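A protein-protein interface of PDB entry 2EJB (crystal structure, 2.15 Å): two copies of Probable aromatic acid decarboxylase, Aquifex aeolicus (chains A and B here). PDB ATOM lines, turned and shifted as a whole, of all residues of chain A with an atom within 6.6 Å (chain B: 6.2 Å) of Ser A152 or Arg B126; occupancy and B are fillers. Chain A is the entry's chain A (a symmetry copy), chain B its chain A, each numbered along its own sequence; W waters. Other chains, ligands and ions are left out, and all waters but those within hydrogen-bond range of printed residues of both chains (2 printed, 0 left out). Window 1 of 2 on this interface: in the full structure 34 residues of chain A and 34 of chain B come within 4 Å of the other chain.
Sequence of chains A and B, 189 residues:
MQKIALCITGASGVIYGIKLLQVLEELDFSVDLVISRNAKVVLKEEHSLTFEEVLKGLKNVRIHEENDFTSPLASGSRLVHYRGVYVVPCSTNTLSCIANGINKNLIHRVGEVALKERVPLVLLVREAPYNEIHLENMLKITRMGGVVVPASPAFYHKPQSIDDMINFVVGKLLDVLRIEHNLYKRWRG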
ATOM      1  N   TYR A  16       9.254  -1.715  14.782  1.00  0.00           N
ATOM      2  CA  TYR A  16       7.879  -2.067  14.428  1.00  0.00           C
ATOM      3  C   TYR A  16       7.890  -3.118  13.321  1.00  0.00           C
ATOM      4  O   TYR A  16       7.102  -4.065  13.338  1.00  0.00           O
ATOM      5  CB  TYR A  16       7.115  -0.832  13.936  1.00  0.00           C
ATOM      6  CG  TYR A  16       6.774   0.170  15.020  1.00  0.00           C
ATOM      7  CD1 TYR A  16       5.880  -0.156  16.040  1.00  0.00           C
ATOM      8  CD2 TYR A  16       7.333   1.446  15.018  1.00  0.00           C
ATOM      9  CE1 TYR A  16       5.548   0.763  17.028  1.00  0.00           C
ATOM     10  CE2 TYR A  16       7.008   2.378  16.006  1.00  0.00           C
ATOM     11  CZ  TYR A  16       6.116   2.028  17.006  1.00  0.00           C
ATOM     12  OH  TYR A  16       5.799   2.936  17.985  1.00  0.00           O
ATOM     13  N   LEU A 124       3.459   2.391   7.435  1.00  0.00           N
ATOM     14  CA  LEU A 124       3.504   2.852   8.817  1.00  0.00           C
ATOM     15  C   LEU A 124       4.410   4.064   8.797  1.00  0.00           C
ATOM     16  O   LEU A 124       5.620   3.934   8.622  1.00  0.00           O
ATOM     17  CB  LEU A 124       4.081   1.794   9.775  1.00  0.00           C
ATOM     18  CG  LEU A 124       3.994   2.257  11.241  1.00  0.00           C
ATOM     19  CD1 LEU A 124       2.548   2.152  11.698  1.00  0.00           C
ATOM     20  CD2 LEU A 124       4.890   1.406  12.138  1.00  0.00           C
ATOM     21  N   VAL A 125       3.824   5.245   8.950  1.00  0.00           N
ATOM     22  CA  VAL A 125       4.598   6.478   8.926  1.00  0.00           C
ATOM     23  C   VAL A 125       4.924   6.959  10.332  1.00  0.00           C
ATOM     24  O   VAL A 125       4.082   6.941  11.228  1.00  0.00           O
ATOM     25  CB  VAL A 125       3.845   7.588   8.163  1.00  0.00           C
ATOM     26  CG1 VAL A 125       4.662   8.869   8.186  1.00  0.00           C
ATOM     27  CG2 VAL A 125       3.594   7.144   6.716  1.00  0.00           C
ATOM     28  N   TYR A 130       4.284  17.140  10.951  1.00  0.00           N
ATOM     29  CA  TYR A 130       4.039  16.882   9.537  1.00  0.00           C
ATOM     30  C   TYR A 130       4.092  18.213   8.791  1.00  0.00           C
ATOM     31  O   TYR A 130       3.645  19.242   9.310  1.00  0.00           O
ATOM     32  CB  TYR A 130       2.634  16.305   9.288  1.00  0.00           C
ATOM     33  CG  TYR A 130       2.337  14.918   9.815  1.00  0.00           C
ATOM     34  CD1 TYR A 130       3.253  13.879   9.678  1.00  0.00           C
ATOM     35  CD2 TYR A 130       1.098  14.631  10.390  1.00  0.00           C
ATOM     36  CE1 TYR A 130       2.946  12.589  10.103  1.00  0.00           C
ATOM     37  CE2 TYR A 130       0.776  13.343  10.815  1.00  0.00           C
ATOM     38  CZ  TYR A 130       1.707  12.329  10.666  1.00  0.00           C
ATOM     39  OH  TYR A 130       1.403  11.054  11.083  1.00  0.00           O
ATOM     40  N   VAL A 149      -0.887   4.159   8.128  1.00  0.00           N
ATOM     41  CA  VAL A 149      -0.983   3.989   9.565  1.00  0.00           C
ATOM     42  C   VAL A 149       0.158   4.747  10.224  1.00  0.00           C
ATOM     43  O   VAL A 149       1.327   4.432  10.000  1.00  0.00           O
ATOM     44  CB  VAL A 149      -0.860   2.503   9.971  1.00  0.00           C
ATOM     45  CG1 VAL A 149      -1.131   2.356  11.462  1.00  0.00           C
ATOM     46  CG2 VAL A 149      -1.825   1.643   9.152  1.00  0.00           C
ATOM     47  N   PRO A 150      -0.160   5.770  11.027  1.00  0.00           N
ATOM     48  CA  PRO A 150       0.913   6.515  11.687  1.00  0.00           C
ATOM     49  C   PRO A 150       1.367   5.690  12.882  1.00  0.00           C
ATOM     50  O   PRO A 150       0.564   4.980  13.476  1.00  0.00           O
ATOM     51  CB  PRO A 150       0.218   7.799  12.120  1.00  0.00           C
ATOM     52  CG  PRO A 150      -1.132   7.291  12.507  1.00  0.00           C
ATOM     53  CD  PRO A 150      -1.474   6.350  11.356  1.00  0.00           C
ATOM     54  N   ALA A 151       2.645   5.756  13.228  1.00  0.00           N
ATOM     55  CA  ALA A 151       3.117   4.999  14.379  1.00  0.00           C
ATOM     56  C   ALA A 151       2.740   5.808  15.618  1.00  0.00           C
ATOM     57  O   ALA A 151       3.594   6.417  16.257  1.00  0.00           O
ATOM     58  CB  ALA A 151       4.628   4.795  14.301  1.00  0.00           C
ATOM     59  N   SER A 152       1.446   5.823  15.936  1.00  0.00           N
ATOM     60  CA  SER A 152       0.939   6.565  17.091  1.00  0.00           C
ATOM     61  C   SER A 152       0.230   5.618  18.052  1.00  0.00           C
ATOM     62  O   SER A 152      -0.998   5.469  18.001  1.00  0.00           O
ATOM     63  CB  SER A 152      -0.046   7.653  16.630  1.00  0.00           C
ATOM     64  OG  SER A 152       0.547   8.520  15.673  1.00  0.00           O
ATOM     65  N   PRO A 153       0.989   4.960  18.946  1.00  0.00           N
ATOM     66  CA  PRO A 153       0.335   4.043  19.878  1.00  0.00           C
ATOM     67  C   PRO A 153      -0.662   4.761  20.772  1.00  0.00           C
ATOM     68  O   PRO A 153      -0.516   5.948  21.053  1.00  0.00           O
ATOM     69  CB  PRO A 153       1.507   3.448  20.655  1.00  0.00           C
ATOM     70  CG  PRO A 153       2.515   4.547  20.626  1.00  0.00           C
ATOM     71  CD  PRO A 153       2.435   5.027  19.208  1.00  0.00           C
ATOM     72  N   ALA A 154      -1.685   4.043  21.203  1.00  0.00           N
ATOM     73  CA  ALA A 154      -2.687   4.628  22.075  1.00  0.00           C
ATOM     74  C   ALA A 154      -2.545   4.038  23.474  1.00  0.00           C
ATOM     75  O   ALA A 154      -1.772   3.107  23.680  1.00  0.00           O
ATOM     76  CB  ALA A 154      -4.053   4.353  21.533  1.00  0.00           C
ATOM     77  N   PHE A 155      -3.290   4.584  24.430  1.00  0.00           N
ATOM     78  CA  PHE A 155      -3.236   4.104  25.802  1.00  0.00           C
ATOM     79  C   PHE A 155      -4.532   3.416  26.224  1.00  0.00           C
ATOM     80  O   PHE A 155      -4.813   3.308  27.414  1.00  0.00           O
ATOM     81  CB  PHE A 155      -2.938   5.266  26.760  1.00  0.00           C
ATOM     82  CG  PHE A 155      -1.603   5.926  26.525  1.00  0.00           C
ATOM     83  CD1 PHE A 155      -1.389   6.726  25.403  1.00  0.00           C
ATOM     84  CD2 PHE A 155      -0.555   5.739  27.420  1.00  0.00           C
ATOM     85  CE1 PHE A 155      -0.150   7.328  25.179  1.00  0.00           C
ATOM     86  CE2 PHE A 155       0.690   6.335  27.206  1.00  0.00           C
ATOM     87  CZ  PHE A 155       0.894   7.133  26.083  1.00  0.00           C
ATOM     88  N   TYR A 156      -5.318   2.951  25.256  1.00  0.00           N
ATOM     89  CA  TYR A 156      -6.574   2.276  25.567  1.00  0.00           C
ATOM     90  C   TYR A 156      -6.328   1.122  26.528  1.00  0.00           C
ATOM     91  O   TYR A 156      -6.925   1.048  27.598  1.00  0.00           O
ATOM     92  CB  TYR A 156      -7.230   1.687  24.309  1.00  0.00           C
ATOM     93  CG  TYR A 156      -7.539   2.642  23.180  1.00  0.00           C
ATOM     94  CD1 TYR A 156      -6.711   2.709  22.066  1.00  0.00           C
ATOM     95  CD2 TYR A 156      -8.673   3.456  23.207  1.00  0.00           C
ATOM     96  CE1 TYR A 156      -7.002   3.559  20.995  1.00  0.00           C
ATOM     97  CE2 TYR A 156      -8.970   4.309  22.147  1.00  0.00           C
ATOM     98  CZ  TYR A 156      -8.130   4.357  21.046  1.00  0.00           C
ATOM     99  OH  TYR A 156      -8.418   5.198  19.993  1.00  0.00           O
ATOM    100  N   PHE A 168       0.750  -2.834  20.069  1.00  0.00           N
ATOM    101  CA  PHE A 168      -0.475  -2.119  19.719  1.00  0.00           C
ATOM    102  C   PHE A 168      -0.425  -1.733  18.246  1.00  0.00           C
ATOM    103  O   PHE A 168      -1.342  -2.027  17.478  1.00  0.00           O
ATOM    104  CB  PHE A 168      -0.633  -0.846  20.554  1.00  0.00           C
ATOM    105  CG  PHE A 168      -1.740   0.051  20.069  1.00  0.00           C
ATOM    106  CD1 PHE A 168      -3.068  -0.221  20.384  1.00  0.00           C
ATOM    107  CD2 PHE A 168      -1.460   1.130  19.234  1.00  0.00           C
ATOM    108  CE1 PHE A 168      -4.104   0.564  19.866  1.00  0.00           C
ATOM    109  CE2 PHE A 168      -2.487   1.919  18.710  1.00  0.00           C
ATOM    110  CZ  PHE A 168      -3.813   1.634  19.027  1.00  0.00           C
ATOM    111  N   VAL A 169       0.657  -1.070  17.855  1.00  0.00           N
ATOM    112  CA  VAL A 169       0.823  -0.637  16.476  1.00  0.00           C
ATOM    113  C   VAL A 169       0.851  -1.838  15.524  1.00  0.00           C
ATOM    114  O   VAL A 169       0.234  -1.804  14.456  1.00  0.00           O
ATOM    115  CB  VAL A 169       2.110   0.188  16.317  1.00  0.00           C
ATOM    116  CG1 VAL A 169       2.266   0.639  14.874  1.00  0.00           C
ATOM    117  CG2 VAL A 169       2.059   1.398  17.249  1.00  0.00           C
ATOM    118  N   LYS A 172      -2.540  -3.087  14.962  1.00  0.00           N
ATOM    119  CA  LYS A 172      -3.286  -2.200  14.083  1.00  0.00           C
ATOM    120  C   LYS A 172      -2.958  -2.538  12.633  1.00  0.00           C
ATOM    121  O   LYS A 172      -3.837  -2.567  11.775  1.00  0.00           O
ATOM    122  CB  LYS A 172      -2.923  -0.738  14.370  1.00  0.00           C
ATOM    123  CG  LYS A 172      -3.875  -0.032  15.324  1.00  0.00           C
ATOM    124  CD  LYS A 172      -5.223   0.186  14.648  1.00  0.00           C
ATOM    125  CE  LYS A 172      -6.161   1.015  15.504  1.00  0.00           C
ATOM    126  NZ  LYS A 172      -7.478   1.220  14.832  1.00  0.00           N
ATOM    127  N   ALA B  11      -9.294  12.323  24.024  1.00  0.00           N
ATOM    128  CA  ALA B  11      -8.670  11.422  23.066  1.00  0.00           C
ATOM    129  C   ALA B  11      -7.637  10.598  23.825  1.00  0.00           C
ATOM    130  O   ALA B  11      -7.078  11.066  24.817  1.00  0.00           O
ATOM    131  CB  ALA B  11      -7.996  12.219  21.951  1.00  0.00           C
ATOM    132  N   SER B  12      -7.393   9.375  23.368  1.00  0.00           N
ATOM    133  CA  SER B  12      -6.420   8.510  24.026  1.00  0.00           C
ATOM    134  C   SER B  12      -5.061   9.189  23.952  1.00  0.00           C
ATOM    135  O   SER B  12      -4.593   9.548  22.869  1.00  0.00           O
ATOM    136  CB  SER B  12      -6.357   7.144  23.336  1.00  0.00           C
ATOM    137  OG  SER B  12      -5.428   6.289  23.978  1.00  0.00           O
ATOM    138  N   GLY B  13      -4.441   9.376  25.109  1.00  0.00           N
ATOM    139  CA  GLY B  13      -3.144  10.022  25.154  1.00  0.00           C
ATOM    140  C   GLY B  13      -3.230  11.330  25.912  1.00  0.00           C
ATOM    141  O   GLY B  13      -2.383  12.212  25.746  1.00  0.00           O
ATOM    142  N   TYR B  16      -0.135  13.011  27.478  1.00  0.00           N
ATOM    143  CA  TYR B  16       0.766  13.946  26.805  1.00  0.00           C
ATOM    144  C   TYR B  16       0.451  15.372  27.254  1.00  0.00           C
ATOM    145  O   TYR B  16       1.354  16.177  27.485  1.00  0.00           O
ATOM    146  CB  TYR B  16       0.600  13.855  25.283  1.00  0.00           C
ATOM    147  CG  TYR B  16       1.156  12.588  24.665  1.00  0.00           C
ATOM    148  CD1 TYR B  16       2.527  12.328  24.676  1.00  0.00           C
ATOM    149  CD2 TYR B  16       0.316  11.659  24.057  1.00  0.00           C
ATOM    150  CE1 TYR B  16       3.047  11.178  24.096  1.00  0.00           C
ATOM    151  CE2 TYR B  16       0.826  10.498  23.471  1.00  0.00           C
ATOM    152  CZ  TYR B  16       2.191  10.267  23.496  1.00  0.00           C
ATOM    153  OH  TYR B  16       2.699   9.124  22.930  1.00  0.00           O
ATOM    154  N   PRO B  89      -4.137  16.382  24.173  1.00  0.00           N
ATOM    155  CA  PRO B  89      -4.186  15.892  22.793  1.00  0.00           C
ATOM    156  C   PRO B  89      -5.396  16.488  22.086  1.00  0.00           C
ATOM    157  O   PRO B  89      -6.335  16.940  22.734  1.00  0.00           O
ATOM    158  CB  PRO B  89      -4.317  14.385  22.970  1.00  0.00           C
ATOM    159  CG  PRO B  89      -5.196  14.289  24.179  1.00  0.00           C
ATOM    160  CD  PRO B  89      -4.605  15.344  25.113  1.00  0.00           C
ATOM    161  N   CYS B  90      -5.366  16.480  20.758  1.00  0.00           N
ATOM    162  CA  CYS B  90      -6.459  17.007  19.956  1.00  0.00           C
ATOM    163  C   CYS B  90      -7.208  15.846  19.301  1.00  0.00           C
ATOM    164  O   CYS B  90      -6.691  15.211  18.383  1.00  0.00           O
ATOM    165  CB  CYS B  90      -5.909  17.943  18.876  1.00  0.00           C
ATOM    166  SG  CYS B  90      -7.172  18.636  17.775  1.00  0.00           S
ATOM    167  N   THR B  92      -9.932  13.730  17.034  1.00  0.00           N
ATOM    168  CA  THR B  92     -10.259  13.885  15.625  1.00  0.00           C
ATOM    169  C   THR B  92     -11.452  14.810  15.470  1.00  0.00           C
ATOM    170  O   THR B  92     -11.558  15.548  14.486  1.00  0.00           O
ATOM    171  CB  THR B  92     -10.568  12.519  14.951  1.00  0.00           C
ATOM    172  OG1 THR B  92     -11.576  11.820  15.695  1.00  0.00           O
ATOM    173  CG2 THR B  92      -9.305  11.670  14.885  1.00  0.00           C
ATOM    174  N   LEU B 124      -1.770  18.041  18.735  1.00  0.00           N
ATOM    175  CA  LEU B 124      -1.128  16.736  18.839  1.00  0.00           C
ATOM    176  C   LEU B 124      -2.209  15.739  18.482  1.00  0.00           C
ATOM    177  O   LEU B 124      -3.143  15.530  19.252  1.00  0.00           O
ATOM    178  CB  LEU B 124      -0.608  16.445  20.258  1.00  0.00           C
ATOM    179  CG  LEU B 124       0.178  15.121  20.307  1.00  0.00           C
ATOM    180  CD1 LEU B 124       1.534  15.338  19.653  1.00  0.00           C
ATOM    181  CD2 LEU B 124       0.362  14.646  21.746  1.00  0.00           C
ATOM    182  N   VAL B 125      -2.097  15.140  17.302  1.00  0.00           N
ATOM    183  CA  VAL B 125      -3.091  14.178  16.848  1.00  0.00           C
ATOM    184  C   VAL B 125      -2.645  12.748  17.114  1.00  0.00           C
ATOM    185  O   VAL B 125      -1.492  12.384  16.892  1.00  0.00           O
ATOM    186  CB  VAL B 125      -3.385  14.355  15.344  1.00  0.00           C
ATOM    187  CG1 VAL B 125      -4.399  13.316  14.895  1.00  0.00           C
ATOM    188  CG2 VAL B 125      -3.922  15.769  15.083  1.00  0.00           C
ATOM    189  N   ARG B 126      -3.584  11.947  17.599  1.00  0.00           N
ATOM    190  CA  ARG B 126      -3.327  10.558  17.929  1.00  0.00           C
ATOM    191  C   ARG B 126      -4.482   9.729  17.377  1.00  0.00           C
ATOM    192  O   ARG B 126      -5.537   9.619  17.999  1.00  0.00           O
ATOM    193  CB  ARG B 126      -3.224  10.423  19.454  1.00  0.00           C
ATOM    194  CG  ARG B 126      -2.738   9.084  19.987  1.00  0.00           C
ATOM    195  CD  ARG B 126      -3.833   8.043  19.941  1.00  0.00           C
ATOM    196  NE  ARG B 126      -3.507   6.979  19.008  1.00  0.00           N
ATOM    197  CZ  ARG B 126      -4.384   6.100  18.543  1.00  0.00           C
ATOM    198  NH1 ARG B 126      -5.654   6.160  18.925  1.00  0.00           N
ATOM    199  NH2 ARG B 126      -3.987   5.165  17.693  1.00  0.00           N
ATOM    200  N   GLU B 127      -4.279   9.171  16.188  1.00  0.00           N
ATOM    201  CA  GLU B 127      -5.287   8.345  15.536  1.00  0.00           C
ATOM    202  C   GLU B 127      -4.600   7.368  14.580  1.00  0.00           C
ATOM    203  O   GLU B 127      -3.495   7.629  14.110  1.00  0.00           O
ATOM    204  CB  GLU B 127      -6.282   9.229  14.772  1.00  0.00           C
ATOM    205  CG  GLU B 127      -7.335   8.450  13.997  1.00  0.00           C
ATOM    206  CD  GLU B 127      -8.176   7.560  14.890  1.00  0.00           C
ATOM    207  OE1 GLU B 127      -9.169   8.059  15.464  1.00  0.00           O
ATOM    208  OE2 GLU B 127      -7.833   6.363  15.024  1.00  0.00           O
ATOM    209  N   ALA B 128      -5.252   6.243  14.301  1.00  0.00           N
ATOM    210  CA  ALA B 128      -4.696   5.237  13.408  1.00  0.00           C
ATOM    211  C   ALA B 128      -5.731   4.170  13.054  1.00  0.00           C
ATOM    212  O   ALA B 128      -6.403   3.636  13.932  1.00  0.00           O
ATOM    213  CB  ALA B 128      -3.473   4.574  14.061  1.00  0.00           C
ATOM    214  N   TYR B 130      -5.287   6.603   9.388  1.00  0.00           N
ATOM    215  CA  TYR B 130      -5.872   7.881   9.003  1.00  0.00           C
ATOM    216  C   TYR B 130      -6.814   7.642   7.826  1.00  0.00           C
ATOM    217  O   TYR B 130      -6.530   6.814   6.953  1.00  0.00           O
ATOM    218  CB  TYR B 130      -4.811   8.880   8.510  1.00  0.00           C
ATOM    219  CG  TYR B 130      -3.805   9.396   9.516  1.00  0.00           C
ATOM    220  CD1 TYR B 130      -4.195   9.787  10.794  1.00  0.00           C
ATOM    221  CD2 TYR B 130      -2.466   9.561   9.158  1.00  0.00           C
ATOM    222  CE1 TYR B 130      -3.276  10.327  11.692  1.00  0.00           C
ATOM    223  CE2 TYR B 130      -1.539  10.103  10.045  1.00  0.00           C
ATOM    224  CZ  TYR B 130      -1.954  10.484  11.309  1.00  0.00           C
ATOM    225  OH  TYR B 130      -1.049  11.019  12.195  1.00  0.00           O
ATOM    226  N   VAL B 149       1.182  17.987  15.022  1.00  0.00           N
ATOM    227  CA  VAL B 149       2.174  17.056  15.525  1.00  0.00           C
ATOM    228  C   VAL B 149       1.487  15.739  15.851  1.00  0.00           C
ATOM    229  O   VAL B 149       0.616  15.688  16.719  1.00  0.00           O
ATOM    230  CB  VAL B 149       2.837  17.576  16.821  1.00  0.00           C
ATOM    231  CG1 VAL B 149       3.979  16.650  17.218  1.00  0.00           C
ATOM    232  CG2 VAL B 149       3.335  19.009  16.629  1.00  0.00           C
ATOM    233  N   PRO B 150       1.851  14.660  15.146  1.00  0.00           N
ATOM    234  CA  PRO B 150       1.218  13.373  15.440  1.00  0.00           C
ATOM    235  C   PRO B 150       1.891  12.813  16.685  1.00  0.00           C
ATOM    236  O   PRO B 150       3.071  13.060  16.906  1.00  0.00           O
ATOM    237  CB  PRO B 150       1.543  12.546  14.203  1.00  0.00           C
ATOM    238  CG  PRO B 150       2.924  13.015  13.884  1.00  0.00           C
ATOM    239  CD  PRO B 150       2.800  14.529  14.026  1.00  0.00           C
ATOM    240  N   ALA B 151       1.153  12.082  17.509  1.00  0.00           N
ATOM    241  CA  ALA B 151       1.763  11.510  18.701  1.00  0.00           C
ATOM    242  C   ALA B 151       2.504  10.253  18.251  1.00  0.00           C
ATOM    243  O   ALA B 151       2.064   9.136  18.507  1.00  0.00           O
ATOM    244  CB  ALA B 151       0.695  11.169  19.737  1.00  0.00           C
ATOM    245  N   SER B 152       3.625  10.450  17.558  1.00  0.00           N
ATOM    246  CA  SER B 152       4.433   9.339  17.053  1.00  0.00           C
ATOM    247  C   SER B 152       5.846   9.420  17.618  1.00  0.00           C
ATOM    248  O   SER B 152       6.753   9.964  16.973  1.00  0.00           O
ATOM    249  CB  SER B 152       4.495   9.385  15.516  1.00  0.00           C
ATOM    250  OG  SER B 152       3.196   9.387  14.943  1.00  0.00           O
ATOM    251  N   PRO B 153       6.060   8.882  18.830  1.00  0.00           N
ATOM    252  CA  PRO B 153       7.406   8.948  19.397  1.00  0.00           C
ATOM    253  C   PRO B 153       8.419   8.210  18.537  1.00  0.00           C
ATOM    254  O   PRO B 153       8.077   7.265  17.832  1.00  0.00           O
ATOM    255  CB  PRO B 153       7.230   8.318  20.778  1.00  0.00           C
ATOM    256  CG  PRO B 153       6.109   7.358  20.562  1.00  0.00           C
ATOM    257  CD  PRO B 153       5.150   8.156  19.730  1.00  0.00           C
HETATM  258  O   HOH W   1       3.410   9.804  12.231  1.00  0.00           O
HETATM  259  O   HOH W   2      -1.381  10.210  14.673  1.00  0.00           O
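O of Val B125 sits at hydrogen-bond distance from N of Ala B151 (2.7 Å). O of Val A125 lies within hydrogen-bond range of N of Ala A151 (2.7 Å).
Water W1 lies within hydrogen-bond range of OH of Tyr A130, OG of Ser B152 and O of Val A125. Water W2 lies within hydrogen-bond range of OH of Tyr B130 (2.6 Å), OG of Ser A152 (2.8 Å), O of Val B125 (3.1 Å) and O of Glu B127 (3.4 Å).
Among the printed residues, pairs that only touch across the chains: Tyr A130 with Pro B150 (3.5 Å), Pro A150 with Glu B127 (2.9 Å), Pro A150 with Ala B128 (3.8 Å), Pro A150 with Tyr B130 (3.5 Å), Ala A151 with Ala B151 (3.8 Å), Pro A153 with Arg B126 (3.8 Å), Ala A154 with Ser B12 (3.4 Å), Ala A154 with Arg B126 (3.5 Å), Phe A155 with Gly B13 (3.7 Å), Phe A155 with Tyr B16 (3.7 Å), Tyr A156 with Ser B12 (3.6 Å) and Phe A168 with Arg B126 (3.7 Å).
Tyr B130 touches its own counterpart, Tyr A130. Ala B151 touches its own counterpart, Ala A151. Ala A151 touches Ser B152, and with the chains exchanged Ser A152 touches Ala B151. Ser B152 touches its own counterpart, Ser A152. Of the 20 pairs that touch across the chains among the printed residues, 7 have their exchanged pair printed and touching as well.
The backbone NH (N) of Phe A155 sits at hydrogen-bond distance from the side-chain hydroxyl (OG) of Ser B12, at 2.8 Å. NH2 of Arg B126 is in hydrogen-bond range of O of Ser A152. The guanidinium group of Arg B126 is in hydrogen-bond range of the side-chain hydroxyl of Tyr A156 (3.1 Å). NZ of Lys A172 is in hydrogen-bond range of O of Ala B128 (2.8 Å). The side-chain hydroxyl (OH) of Tyr A130 sits at hydrogen-bond distance from the side-chain hydroxyl (OH) of Tyr B130. The side-chain hydroxyl (OG) of Ser A152 lies close to the backbone carbonyl oxygen (O) of Ala B151 (3.3 Å). The side-chain hydroxyl (OG) of Ser B152 lies close to the backbone carbonyl oxygen (O) of Ala A151, 3.3 Å away. OG of Ser B152 sits at hydrogen-bond distance from OG of Ser A152 (2.9 Å).
Ser A152 touches just these residues of chain B: Arg B126 (3.0 Å), Ala B151 (3.1 Å) and Ser B152 (2.9 Å). Of the printed residues of chain B, Pro A153 touches Arg B126 (3.8 Å). Printed residues of chain B within 4 Å of Phe A155: Ser B12, Gly B13 and Tyr B16. Leu B124 touches none of the printed residues of chain A. Printed residues of chain A within 4 Å of Arg B126: Ser A152 (3.0 Å), Pro A153 (3.8 Å), Ala A154 (3.5 Å), Tyr A156 (3.1 Å) and Phe A168 (3.7 Å). Of the printed residues of chain A, Glu B127 touches Pro A150 (2.9 Å). The nearest residue of chain B that does not touch Ser A152 is Glu B127 (4.3 Å). The nearest residue of chain A that does not touch Arg B126 is Lys A172 (5.2 Å). The nearest printed residue of chain B that does not touch Phe A168 is Ala B128 (5.4 Å).
Of the 15 printed residues of chain A, 10 touch a printed residue of chain B. Printed residues of chain A that touch a printed residue of chain B: Tyr A130, Pro A150, Ala A151, Ser A152, Pro A153, Ala A154, Phe A155, Tyr A156, Phe A168 and Lys A172. Along chain A the printed residues that touch a printed residue of chain B span positions 130 to 172. Hydrophobic or aromatic side chains of chain B that line the printed part of chain A: Tyr B16, Ala B128, Tyr B130 and Pro B150.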
